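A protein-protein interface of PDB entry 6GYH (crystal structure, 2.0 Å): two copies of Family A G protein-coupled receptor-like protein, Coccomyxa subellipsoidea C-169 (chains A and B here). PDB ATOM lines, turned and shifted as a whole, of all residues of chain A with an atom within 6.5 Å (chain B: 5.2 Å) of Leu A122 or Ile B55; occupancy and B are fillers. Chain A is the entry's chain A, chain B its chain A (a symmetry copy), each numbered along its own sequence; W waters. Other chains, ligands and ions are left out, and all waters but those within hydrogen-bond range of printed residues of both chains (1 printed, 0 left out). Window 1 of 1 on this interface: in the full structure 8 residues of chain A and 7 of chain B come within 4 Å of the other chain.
Water W1 lies within hydrogen-bond range of OH of Tyr A137 (2.7 Å) and O of Ala B59 (3.3 Å).
Leu A122 touches just one residue of chain B: Ile B55. Of chain A, only Leu A122 (3.7 Å) and Phe A125 (3.9 Å) come within 4 Å of Ile B55. Printed residues of chain A within 4 Å of Tyr B58: Gly A136 (3.3 Å) and Tyr A137 (3.7 Å). Of the printed residues of chain B, Phe A125 touches Ile B55. Of the printed residues of chain B, Tyr A137 touches Tyr B58 (3.7 Å) and Ala B59 (3.1 Å). Of the printed residues of chain A, Ala B59 touches Tyr A137. Of the printed residues of chain B, Gly A136 touches Tyr B58 (3.3 Å). Gly A123 touches none of the printed residues of chain B. Tyr A138 touches none of the printed residues of chain B. The nearest residue of chain A that does not touch Ile B55 is Tyr A137 (5.0 Å). The nearest printed residue of chain A that does not touch Tyr B58 is Arg A134 (4.9 Å).
No position is printed for both chains. Of the 5 pairs that touch across the chains among the printed residues, none has its exchanged pair printed and touching as well.
Printed residues of chain A that touch a printed residue of chain B: Leu A122, Phe A125, Gly A136 and Tyr A137. Hydrophobic or aromatic side chains of chain A within 4 Å of the printed part of chain B: Leu A122, Phe A125 and Tyr A137. Of the 11 printed residues of chain B, 3 touch a printed residue of chain A. Printed residues of chain B that touch a printed residue of chain A: Ile B55, Tyr B58 and Ala B59. Hydrophobic or aromatic side chains of chain B within 4 Å of the printed part of chain A: Ile B55, Tyr B58 and Ala B59. Among the printed residues, no Asp or Glu carboxylate lies within 4 Å of a Lys or Arg side-chain nitrogen of the other chain.
Among the printed residues, pairs that only touch across the chains: Leu A122 with Ile B55, Phe A125 with Ile B55, Gly A136 with Tyr B58, Tyr A137 with Tyr B58 and Tyr A137 with Ala B59.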
ATOM      1  N   TYR A  84      19.411  21.743   1.658  1.00  0.00           N
ATOM      2  CA  TYR A  84      19.215  20.669   0.693  1.00  0.00           C
ATOM      3  C   TYR A  84      17.744  20.281   0.572  1.00  0.00           C
ATOM      4  O   TYR A  84      17.288  19.903  -0.528  1.00  0.00           O
ATOM      5  CB  TYR A  84      20.062  19.434   1.048  1.00  0.00           C
ATOM      6  CG  TYR A  84      21.535  19.733   0.983  1.00  0.00           C
ATOM      7  CD1 TYR A  84      22.192  20.291   2.094  1.00  0.00           C
ATOM      8  CD2 TYR A  84      22.276  19.482  -0.173  1.00  0.00           C
ATOM      9  CE1 TYR A  84      23.527  20.585   2.054  1.00  0.00           C
ATOM     10  CE2 TYR A  84      23.631  19.780  -0.218  1.00  0.00           C
ATOM     11  CZ  TYR A  84      24.251  20.327   0.914  1.00  0.00           C
ATOM     12  OH  TYR A  84      25.577  20.663   0.972  1.00  0.00           O
ATOM     13  N   VAL A 117      17.217  16.470  -9.027  1.00  0.00           N
ATOM     14  CA  VAL A 117      17.012  15.941  -7.681  1.00  0.00           C
ATOM     15  C   VAL A 117      18.182  15.025  -7.256  1.00  0.00           C
ATOM     16  O   VAL A 117      18.604  15.083  -6.100  1.00  0.00           O
ATOM     17  CB  VAL A 117      15.630  15.277  -7.428  1.00  0.00           C
ATOM     18  CG1 VAL A 117      14.491  16.199  -7.855  1.00  0.00           C
ATOM     19  CG2 VAL A 117      15.513  13.974  -8.128  1.00  0.00           C
ATOM     20  N   ALA A 118      18.683  14.211  -8.199  1.00  0.00           N
ATOM     21  CA  ALA A 118      19.883  13.415  -7.980  1.00  0.00           C
ATOM     22  C   ALA A 118      21.086  14.287  -7.599  1.00  0.00           C
ATOM     23  O   ALA A 118      21.821  13.933  -6.676  1.00  0.00           O
ATOM     24  CB  ALA A 118      20.217  12.583  -9.206  1.00  0.00           C
ATOM     25  N   MET A 119      21.267  15.402  -8.326  1.00  0.00           N
ATOM     26  CA  MET A 119      22.304  16.392  -8.043  1.00  0.00           C
ATOM     27  C   MET A 119      22.266  16.873  -6.576  1.00  0.00           C
ATOM     28  O   MET A 119      23.284  16.864  -5.870  1.00  0.00           O
ATOM     29  CB  MET A 119      22.134  17.600  -8.976  1.00  0.00           C
ATOM     30  CG  MET A 119      23.136  18.729  -8.825  1.00  0.00           C
ATOM     31  SD  MET A 119      22.796  20.128  -9.901  1.00  0.00           S
ATOM     32  CE  MET A 119      21.399  20.869  -9.068  1.00  0.00           C
ATOM     33  N   ILE A 120      21.081  17.270  -6.144  1.00  0.00           N
ATOM     34  CA  ILE A 120      20.867  17.793  -4.806  1.00  0.00           C
ATOM     35  C   ILE A 120      21.092  16.702  -3.749  1.00  0.00           C
ATOM     36  O   ILE A 120      21.819  16.930  -2.780  1.00  0.00           O
ATOM     37  CB  ILE A 120      19.466  18.407  -4.651  1.00  0.00           C
ATOM     38  CG1 ILE A 120      19.276  19.587  -5.636  1.00  0.00           C
ATOM     39  CG2 ILE A 120      19.197  18.864  -3.203  1.00  0.00           C
ATOM     40  CD1 ILE A 120      20.310  20.682  -5.538  1.00  0.00           C
ATOM     41  N   MET A 121      20.456  15.545  -3.959  1.00  0.00           N
ATOM     42  CA  MET A 121      20.531  14.445  -3.038  1.00  0.00           C
ATOM     43  C   MET A 121      21.943  13.938  -2.838  1.00  0.00           C
ATOM     44  O   MET A 121      22.303  13.633  -1.709  1.00  0.00           O
ATOM     45  CB  MET A 121      19.593  13.302  -3.452  1.00  0.00           C
ATOM     46  CG  MET A 121      18.118  13.688  -3.221  1.00  0.00           C
ATOM     47  SD  MET A 121      17.631  13.928  -1.477  1.00  0.00           S
ATOM     48  CE  MET A 121      17.660  15.695  -1.154  1.00  0.00           C
ATOM     49  N   LEU A 122      22.721  13.842  -3.924  1.00  0.00           N
ATOM     50  CA  LEU A 122      24.098  13.396  -3.831  1.00  0.00           C
ATOM     51  C   LEU A 122      24.966  14.445  -3.128  1.00  0.00           C
ATOM     52  O   LEU A 122      25.871  14.080  -2.402  1.00  0.00           O
ATOM     53  CB  LEU A 122      24.690  13.009  -5.191  1.00  0.00           C
ATOM     54  CG  LEU A 122      24.161  11.778  -5.911  1.00  0.00           C
ATOM     55  CD1 LEU A 122      24.839  11.647  -7.272  1.00  0.00           C
ATOM     56  CD2 LEU A 122      24.339  10.493  -5.169  1.00  0.00           C
ATOM     57  N   GLY A 123      24.697  15.730  -3.347  1.00  0.00           N
ATOM     58  CA  GLY A 123      25.313  16.796  -2.557  1.00  0.00           C
ATOM     59  C   GLY A 123      25.049  16.645  -1.058  1.00  0.00           C
ATOM     60  O   GLY A 123      25.971  16.816  -0.265  1.00  0.00           O
ATOM     61  N   LEU A 124      23.792  16.327  -0.696  1.00  0.00           N
ATOM     62  CA  LEU A 124      23.389  16.104   0.691  1.00  0.00           C
ATOM     63  C   LEU A 124      24.178  14.963   1.298  1.00  0.00           C
ATOM     64  O   LEU A 124      24.738  15.118   2.368  1.00  0.00           O
ATOM     65  CB  LEU A 124      21.910  15.812   0.835  1.00  0.00           C
ATOM     66  CG  LEU A 124      21.408  15.472   2.249  1.00  0.00           C
ATOM     67  CD1 LEU A 124      21.671  16.623   3.208  1.00  0.00           C
ATOM     68  CD2 LEU A 124      19.946  15.171   2.185  1.00  0.00           C
ATOM     69  N   PHE A 125      24.210  13.839   0.591  1.00  0.00           N
ATOM     70  CA  PHE A 125      24.934  12.653   1.030  1.00  0.00           C
ATOM     71  C   PHE A 125      26.435  12.921   1.221  1.00  0.00           C
ATOM     72  O   PHE A 125      27.020  12.490   2.209  1.00  0.00           O
ATOM     73  CB  PHE A 125      24.732  11.491   0.046  1.00  0.00           C
ATOM     74  CG  PHE A 125      23.278  11.027  -0.125  1.00  0.00           C
ATOM     75  CD1 PHE A 125      22.271  11.369   0.771  1.00  0.00           C
ATOM     76  CD2 PHE A 125      22.936  10.195  -1.217  1.00  0.00           C
ATOM     77  CE1 PHE A 125      20.973  10.926   0.586  1.00  0.00           C
ATOM     78  CE2 PHE A 125      21.626   9.747  -1.400  1.00  0.00           C
ATOM     79  CZ  PHE A 125      20.651  10.110  -0.485  1.00  0.00           C
ATOM     80  N   GLY A 126      27.032  13.640   0.272  1.00  0.00           N
ATOM     81  CA  GLY A 126      28.394  14.104   0.379  1.00  0.00           C
ATOM     82  C   GLY A 126      28.604  14.990   1.589  1.00  0.00           C
ATOM     83  O   GLY A 126      29.613  14.860   2.300  1.00  0.00           O
ATOM     84  N   ALA A 127      27.656  15.899   1.822  1.00  0.00           N
ATOM     85  CA  ALA A 127      27.726  16.785   2.974  1.00  0.00           C
ATOM     86  C   ALA A 127      27.626  16.047   4.328  1.00  0.00           C
ATOM     87  O   ALA A 127      28.272  16.456   5.300  1.00  0.00           O
ATOM     88  CB  ALA A 127      26.679  17.889   2.883  1.00  0.00           C
ATOM     89  N   ARG A 134      32.900  11.415   0.198  1.00  0.00           N
ATOM     90  CA  ARG A 134      32.298  12.722  -0.058  1.00  0.00           C
ATOM     91  C   ARG A 134      32.552  13.241  -1.486  1.00  0.00           C
ATOM     92  O   ARG A 134      31.655  13.839  -2.079  1.00  0.00           O
ATOM     93  CB  ARG A 134      32.783  13.769   0.972  1.00  0.00           C
ATOM     94  CG  ARG A 134      34.264  14.190   0.854  1.00  0.00           C
ATOM     95  CD  ARG A 134      34.891  14.890   2.076  1.00  0.00           C
ATOM     96  NE  ARG A 134      34.041  15.901   2.715  1.00  0.00           N
ATOM     97  CZ  ARG A 134      33.199  15.695   3.722  1.00  0.00           C
ATOM     98  NH1 ARG A 134      33.048  14.491   4.278  1.00  0.00           N
ATOM     99  NH2 ARG A 134      32.473  16.717   4.191  1.00  0.00           N
ATOM    100  N   GLY A 136      33.289  11.409  -4.321  1.00  0.00           N
ATOM    101  CA  GLY A 136      32.556  10.615  -5.324  1.00  0.00           C
ATOM    102  C   GLY A 136      31.120  11.135  -5.480  1.00  0.00           C
ATOM    103  O   GLY A 136      30.633  11.317  -6.608  1.00  0.00           O
ATOM    104  N   TYR A 137      30.442  11.381  -4.347  1.00  0.00           N
ATOM    105  CA  TYR A 137      29.154  12.065  -4.344  1.00  0.00           C
ATOM    106  C   TYR A 137      29.209  13.386  -5.115  1.00  0.00           C
ATOM    107  O   TYR A 137      28.349  13.652  -5.999  1.00  0.00           O
ATOM    108  CB  TYR A 137      28.679  12.386  -2.933  1.00  0.00           C
ATOM    109  CG  TYR A 137      28.197  11.204  -2.122  1.00  0.00           C
ATOM    110  CD1 TYR A 137      27.107  10.438  -2.555  1.00  0.00           C
ATOM    111  CD2 TYR A 137      28.815  10.855  -0.906  1.00  0.00           C
ATOM    112  CE1 TYR A 137      26.658   9.355  -1.824  1.00  0.00           C
ATOM    113  CE2 TYR A 137      28.367   9.770  -0.155  1.00  0.00           C
ATOM    114  CZ  TYR A 137      27.289   9.031  -0.610  1.00  0.00           C
ATOM    115  OH  TYR A 137      26.819   7.975   0.109  1.00  0.00           O
ATOM    116  N   TYR A 138      30.211  14.200  -4.788  1.00  0.00           N
ATOM    117  CA  TYR A 138      30.362  15.521  -5.405  1.00  0.00           C
ATOM    118  C   TYR A 138      30.530  15.462  -6.920  1.00  0.00           C
ATOM    119  O   TYR A 138      29.857  16.192  -7.641  1.00  0.00           O
ATOM    120  CB  TYR A 138      31.574  16.229  -4.820  1.00  0.00           C
ATOM    121  CG  TYR A 138      31.848  17.604  -5.355  1.00  0.00           C
ATOM    122  CD1 TYR A 138      31.045  18.688  -4.987  1.00  0.00           C
ATOM    123  CD2 TYR A 138      32.905  17.834  -6.237  1.00  0.00           C
ATOM    124  CE1 TYR A 138      31.297  19.971  -5.464  1.00  0.00           C
ATOM    125  CE2 TYR A 138      33.174  19.112  -6.734  1.00  0.00           C
ATOM    126  CZ  TYR A 138      32.366  20.182  -6.340  1.00  0.00           C
ATOM    127  OH  TYR A 138      32.639  21.456  -6.816  1.00  0.00           O
ATOM    128  N   VAL A 140      29.853  12.962  -9.104  1.00  0.00           N
ATOM    129  CA  VAL A 140      28.683  12.413  -9.802  1.00  0.00           C
ATOM    130  C   VAL A 140      27.540  13.440  -9.818  1.00  0.00           C
ATOM    131  O   VAL A 140      26.812  13.561 -10.837  1.00  0.00           O
ATOM    132  CB  VAL A 140      28.230  11.057  -9.202  1.00  0.00           C
ATOM    133  CG1 VAL A 140      26.925  10.555  -9.841  1.00  0.00           C
ATOM    134  CG2 VAL A 140      29.329  10.022  -9.423  1.00  0.00           C
ATOM    135  N   SER A 141      27.390  14.170  -8.703  1.00  0.00           N
ATOM    136  CA  SER A 141      26.458  15.283  -8.648  1.00  0.00           C
ATOM    137  C   SER A 141      26.772  16.382  -9.678  1.00  0.00           C
ATOM    138  O   SER A 141      25.841  16.922 -10.288  1.00  0.00           O
ATOM    139  CB  SER A 141      26.393  15.855  -7.259  1.00  0.00           C
ATOM    140  OG  SER A 141      25.462  16.909  -7.193  1.00  0.00           O
ATOM    141  N   PHE A 144      25.498  15.095 -13.040  1.00  0.00           N
ATOM    142  CA  PHE A 144      24.062  15.380 -13.072  1.00  0.00           C
ATOM    143  C   PHE A 144      23.737  16.857 -13.295  1.00  0.00           C
ATOM    144  O   PHE A 144      22.782  17.146 -13.985  1.00  0.00           O
ATOM    145  CB  PHE A 144      23.321  14.872 -11.825  1.00  0.00           C
ATOM    146  CG  PHE A 144      23.060  13.388 -11.828  1.00  0.00           C
ATOM    147  CD1 PHE A 144      22.145  12.821 -12.738  1.00  0.00           C
ATOM    148  CD2 PHE A 144      23.699  12.549 -10.910  1.00  0.00           C
ATOM    149  CE1 PHE A 144      21.891  11.456 -12.732  1.00  0.00           C
ATOM    150  CE2 PHE A 144      23.456  11.188 -10.911  1.00  0.00           C
ATOM    151  CZ  PHE A 144      22.562  10.640 -11.816  1.00  0.00           C
ATOM    152  N   TRP A 189      30.227  24.734  -2.284  1.00  0.00           N
ATOM    153  CA  TRP A 189      30.196  23.430  -1.608  1.00  0.00           C
ATOM    154  C   TRP A 189      31.590  22.815  -1.451  1.00  0.00           C
ATOM    155  O   TRP A 189      31.921  22.328  -0.369  1.00  0.00           O
ATOM    156  CB  TRP A 189      29.289  22.465  -2.351  1.00  0.00           C
ATOM    157  CG  TRP A 189      28.934  21.205  -1.655  1.00  0.00           C
ATOM    158  CD1 TRP A 189      27.755  20.943  -1.047  1.00  0.00           C
ATOM    159  CD2 TRP A 189      29.722  20.014  -1.533  1.00  0.00           C
ATOM    160  NE1 TRP A 189      27.740  19.662  -0.549  1.00  0.00           N
ATOM    161  CE2 TRP A 189      28.932  19.069  -0.835  1.00  0.00           C
ATOM    162  CE3 TRP A 189      31.020  19.649  -1.939  1.00  0.00           C
ATOM    163  CZ2 TRP A 189      29.386  17.794  -0.537  1.00  0.00           C
ATOM    164  CZ3 TRP A 189      31.474  18.376  -1.661  1.00  0.00           C
ATOM    165  CH2 TRP A 189      30.661  17.454  -0.954  1.00  0.00           C
ATOM    166  N   VAL B  50      18.234   0.415 -11.137  1.00  0.00           N
ATOM    167  CA  VAL B  50      19.672   0.159 -10.949  1.00  0.00           C
ATOM    168  C   VAL B  50      20.492   1.426 -10.635  1.00  0.00           C
ATOM    169  O   VAL B  50      21.545   1.317 -10.007  1.00  0.00           O
ATOM    170  CB  VAL B  50      20.321  -0.618 -12.130  1.00  0.00           C
ATOM    171  CG1 VAL B  50      19.851  -2.060 -12.124  1.00  0.00           C
ATOM    172  CG2 VAL B  50      20.087   0.067 -13.481  1.00  0.00           C
ATOM    173  N   THR B  51      20.036   2.600 -11.080  1.00  0.00           N
ATOM    174  CA  THR B  51      20.682   3.859 -10.693  1.00  0.00           C
ATOM    175  C   THR B  51      20.529   4.123  -9.178  1.00  0.00           C
ATOM    176  O   THR B  51      21.512   4.480  -8.505  1.00  0.00           O
ATOM    177  CB  THR B  51      20.152   5.051 -11.514  1.00  0.00           C
ATOM    178  OG1 THR B  51      20.434   4.808 -12.903  1.00  0.00           O
ATOM    179  CG2 THR B  51      20.795   6.367 -11.086  1.00  0.00           C
ATOM    180  N   ILE B  52      19.307   3.952  -8.671  1.00  0.00           N
ATOM    181  CA  ILE B  52      18.996   4.165  -7.263  1.00  0.00           C
ATOM    182  C   ILE B  52      19.736   3.132  -6.390  1.00  0.00           C
ATOM    183  O   ILE B  52      20.336   3.500  -5.357  1.00  0.00           O
ATOM    184  CB  ILE B  52      17.477   4.135  -7.003  1.00  0.00           C
ATOM    185  CG1 ILE B  52      16.807   5.392  -7.609  1.00  0.00           C
ATOM    186  CG2 ILE B  52      17.148   4.016  -5.509  1.00  0.00           C
ATOM    187  CD1 ILE B  52      15.292   5.286  -7.699  1.00  0.00           C
ATOM    188  N   ALA B  53      19.679   1.867  -6.799  1.00  0.00           N
ATOM    189  CA  ALA B  53      20.451   0.820  -6.143  1.00  0.00           C
ATOM    190  C   ALA B  53      21.976   1.089  -6.170  1.00  0.00           C
ATOM    191  O   ALA B  53      22.653   0.862  -5.164  1.00  0.00           O
ATOM    192  CB  ALA B  53      20.132  -0.529  -6.732  1.00  0.00           C
ATOM    193  N   ALA B  54      22.498   1.585  -7.297  1.00  0.00           N
ATOM    194  CA  ALA B  54      23.904   1.994  -7.371  1.00  0.00           C
ATOM    195  C   ALA B  54      24.218   3.072  -6.337  1.00  0.00           C
ATOM    196  O   ALA B  54      25.227   2.960  -5.635  1.00  0.00           O
ATOM    197  CB  ALA B  54      24.313   2.447  -8.767  1.00  0.00           C
ATOM    198  N   ILE B  55      23.344   4.074  -6.210  1.00  0.00           N
ATOM    199  CA  ILE B  55      23.536   5.158  -5.217  1.00  0.00           C
ATOM    200  C   ILE B  55      23.536   4.602  -3.775  1.00  0.00           C
ATOM    201  O   ILE B  55      24.464   4.893  -2.989  1.00  0.00           O
ATOM    202  CB  ILE B  55      22.526   6.313  -5.395  1.00  0.00           C
ATOM    203  CG1 ILE B  55      22.772   7.014  -6.746  1.00  0.00           C
ATOM    204  CG2 ILE B  55      22.642   7.347  -4.254  1.00  0.00           C
ATOM    205  CD1 ILE B  55      21.609   7.828  -7.221  1.00  0.00           C
ATOM    206  N   ALA B  56      22.522   3.789  -3.459  1.00  0.00           N
ATOM    207  CA  ALA B  56      22.439   3.122  -2.151  1.00  0.00           C
ATOM    208  C   ALA B  56      23.673   2.228  -1.831  1.00  0.00           C
ATOM    209  O   ALA B  56      24.225   2.306  -0.712  1.00  0.00           O
ATOM    210  CB  ALA B  56      21.181   2.304  -2.050  1.00  0.00           C
ATOM    211  N   TYR B  57      24.095   1.410  -2.805  1.00  0.00           N
ATOM    212  CA  TYR B  57      25.266   0.550  -2.620  1.00  0.00           C
ATOM    213  C   TYR B  57      26.582   1.321  -2.456  1.00  0.00           C
ATOM    214  O   TYR B  57      27.426   0.928  -1.617  1.00  0.00           O
ATOM    215  CB  TYR B  57      25.364  -0.561  -3.683  1.00  0.00           C
ATOM    216  CG  TYR B  57      24.570  -1.777  -3.241  1.00  0.00           C
ATOM    217  CD1 TYR B  57      25.137  -2.717  -2.355  1.00  0.00           C
ATOM    218  CD2 TYR B  57      23.240  -1.971  -3.638  1.00  0.00           C
ATOM    219  CE1 TYR B  57      24.411  -3.820  -1.917  1.00  0.00           C
ATOM    220  CE2 TYR B  57      22.515  -3.082  -3.203  1.00  0.00           C
ATOM    221  CZ  TYR B  57      23.113  -3.998  -2.348  1.00  0.00           C
ATOM    222  OH  TYR B  57      22.419  -5.078  -1.921  1.00  0.00           O
ATOM    223  N   TYR B  58      26.767   2.394  -3.224  1.00  0.00           N
ATOM    224  CA  TYR B  58      27.884   3.294  -2.995  1.00  0.00           C
ATOM    225  C   TYR B  58      27.881   3.817  -1.534  1.00  0.00           C
ATOM    226  O   TYR B  58      28.928   3.793  -0.862  1.00  0.00           O
ATOM    227  CB  TYR B  58      27.852   4.469  -3.961  1.00  0.00           C
ATOM    228  CG  TYR B  58      28.995   5.421  -3.781  1.00  0.00           C
ATOM    229  CD1 TYR B  58      30.234   5.165  -4.361  1.00  0.00           C
ATOM    230  CD2 TYR B  58      28.852   6.574  -3.002  1.00  0.00           C
ATOM    231  CE1 TYR B  58      31.308   6.036  -4.188  1.00  0.00           C
ATOM    232  CE2 TYR B  58      29.911   7.443  -2.808  1.00  0.00           C
ATOM    233  CZ  TYR B  58      31.143   7.176  -3.412  1.00  0.00           C
ATOM    234  OH  TYR B  58      32.182   8.051  -3.232  1.00  0.00           O
ATOM    235  N   ALA B  59      26.706   4.273  -1.079  1.00  0.00           N
ATOM    236  CA  ALA B  59      26.550   4.878   0.226  1.00  0.00           C
ATOM    237  C   ALA B  59      26.949   3.908   1.333  1.00  0.00           C
ATOM    238  O   ALA B  59      27.686   4.254   2.222  1.00  0.00           O
ATOM    239  CB  ALA B  59      25.118   5.367   0.444  1.00  0.00           C
ATOM    240  N   MET B  60      26.439   2.684   1.228  1.00  0.00           N
ATOM    241  CA  MET B  60      26.712   1.618   2.187  1.00  0.00           C
ATOM    242  C   MET B  60      28.187   1.173   2.126  1.00  0.00           C
ATOM    243  O   MET B  60      28.809   0.928   3.168  1.00  0.00           O
ATOM    244  CB  MET B  60      25.742   0.464   1.959  1.00  0.00           C
ATOM    245  CG  MET B  60      24.298   0.840   2.236  1.00  0.00           C
ATOM    246  SD  MET B  60      23.242  -0.621   2.329  1.00  0.00           S
ATOM    247  CE  MET B  60      23.288  -1.186   0.636  1.00  0.00           C
HETATM  248  O   HOH W   1      27.901   7.543   2.545  1.00  0.00           O
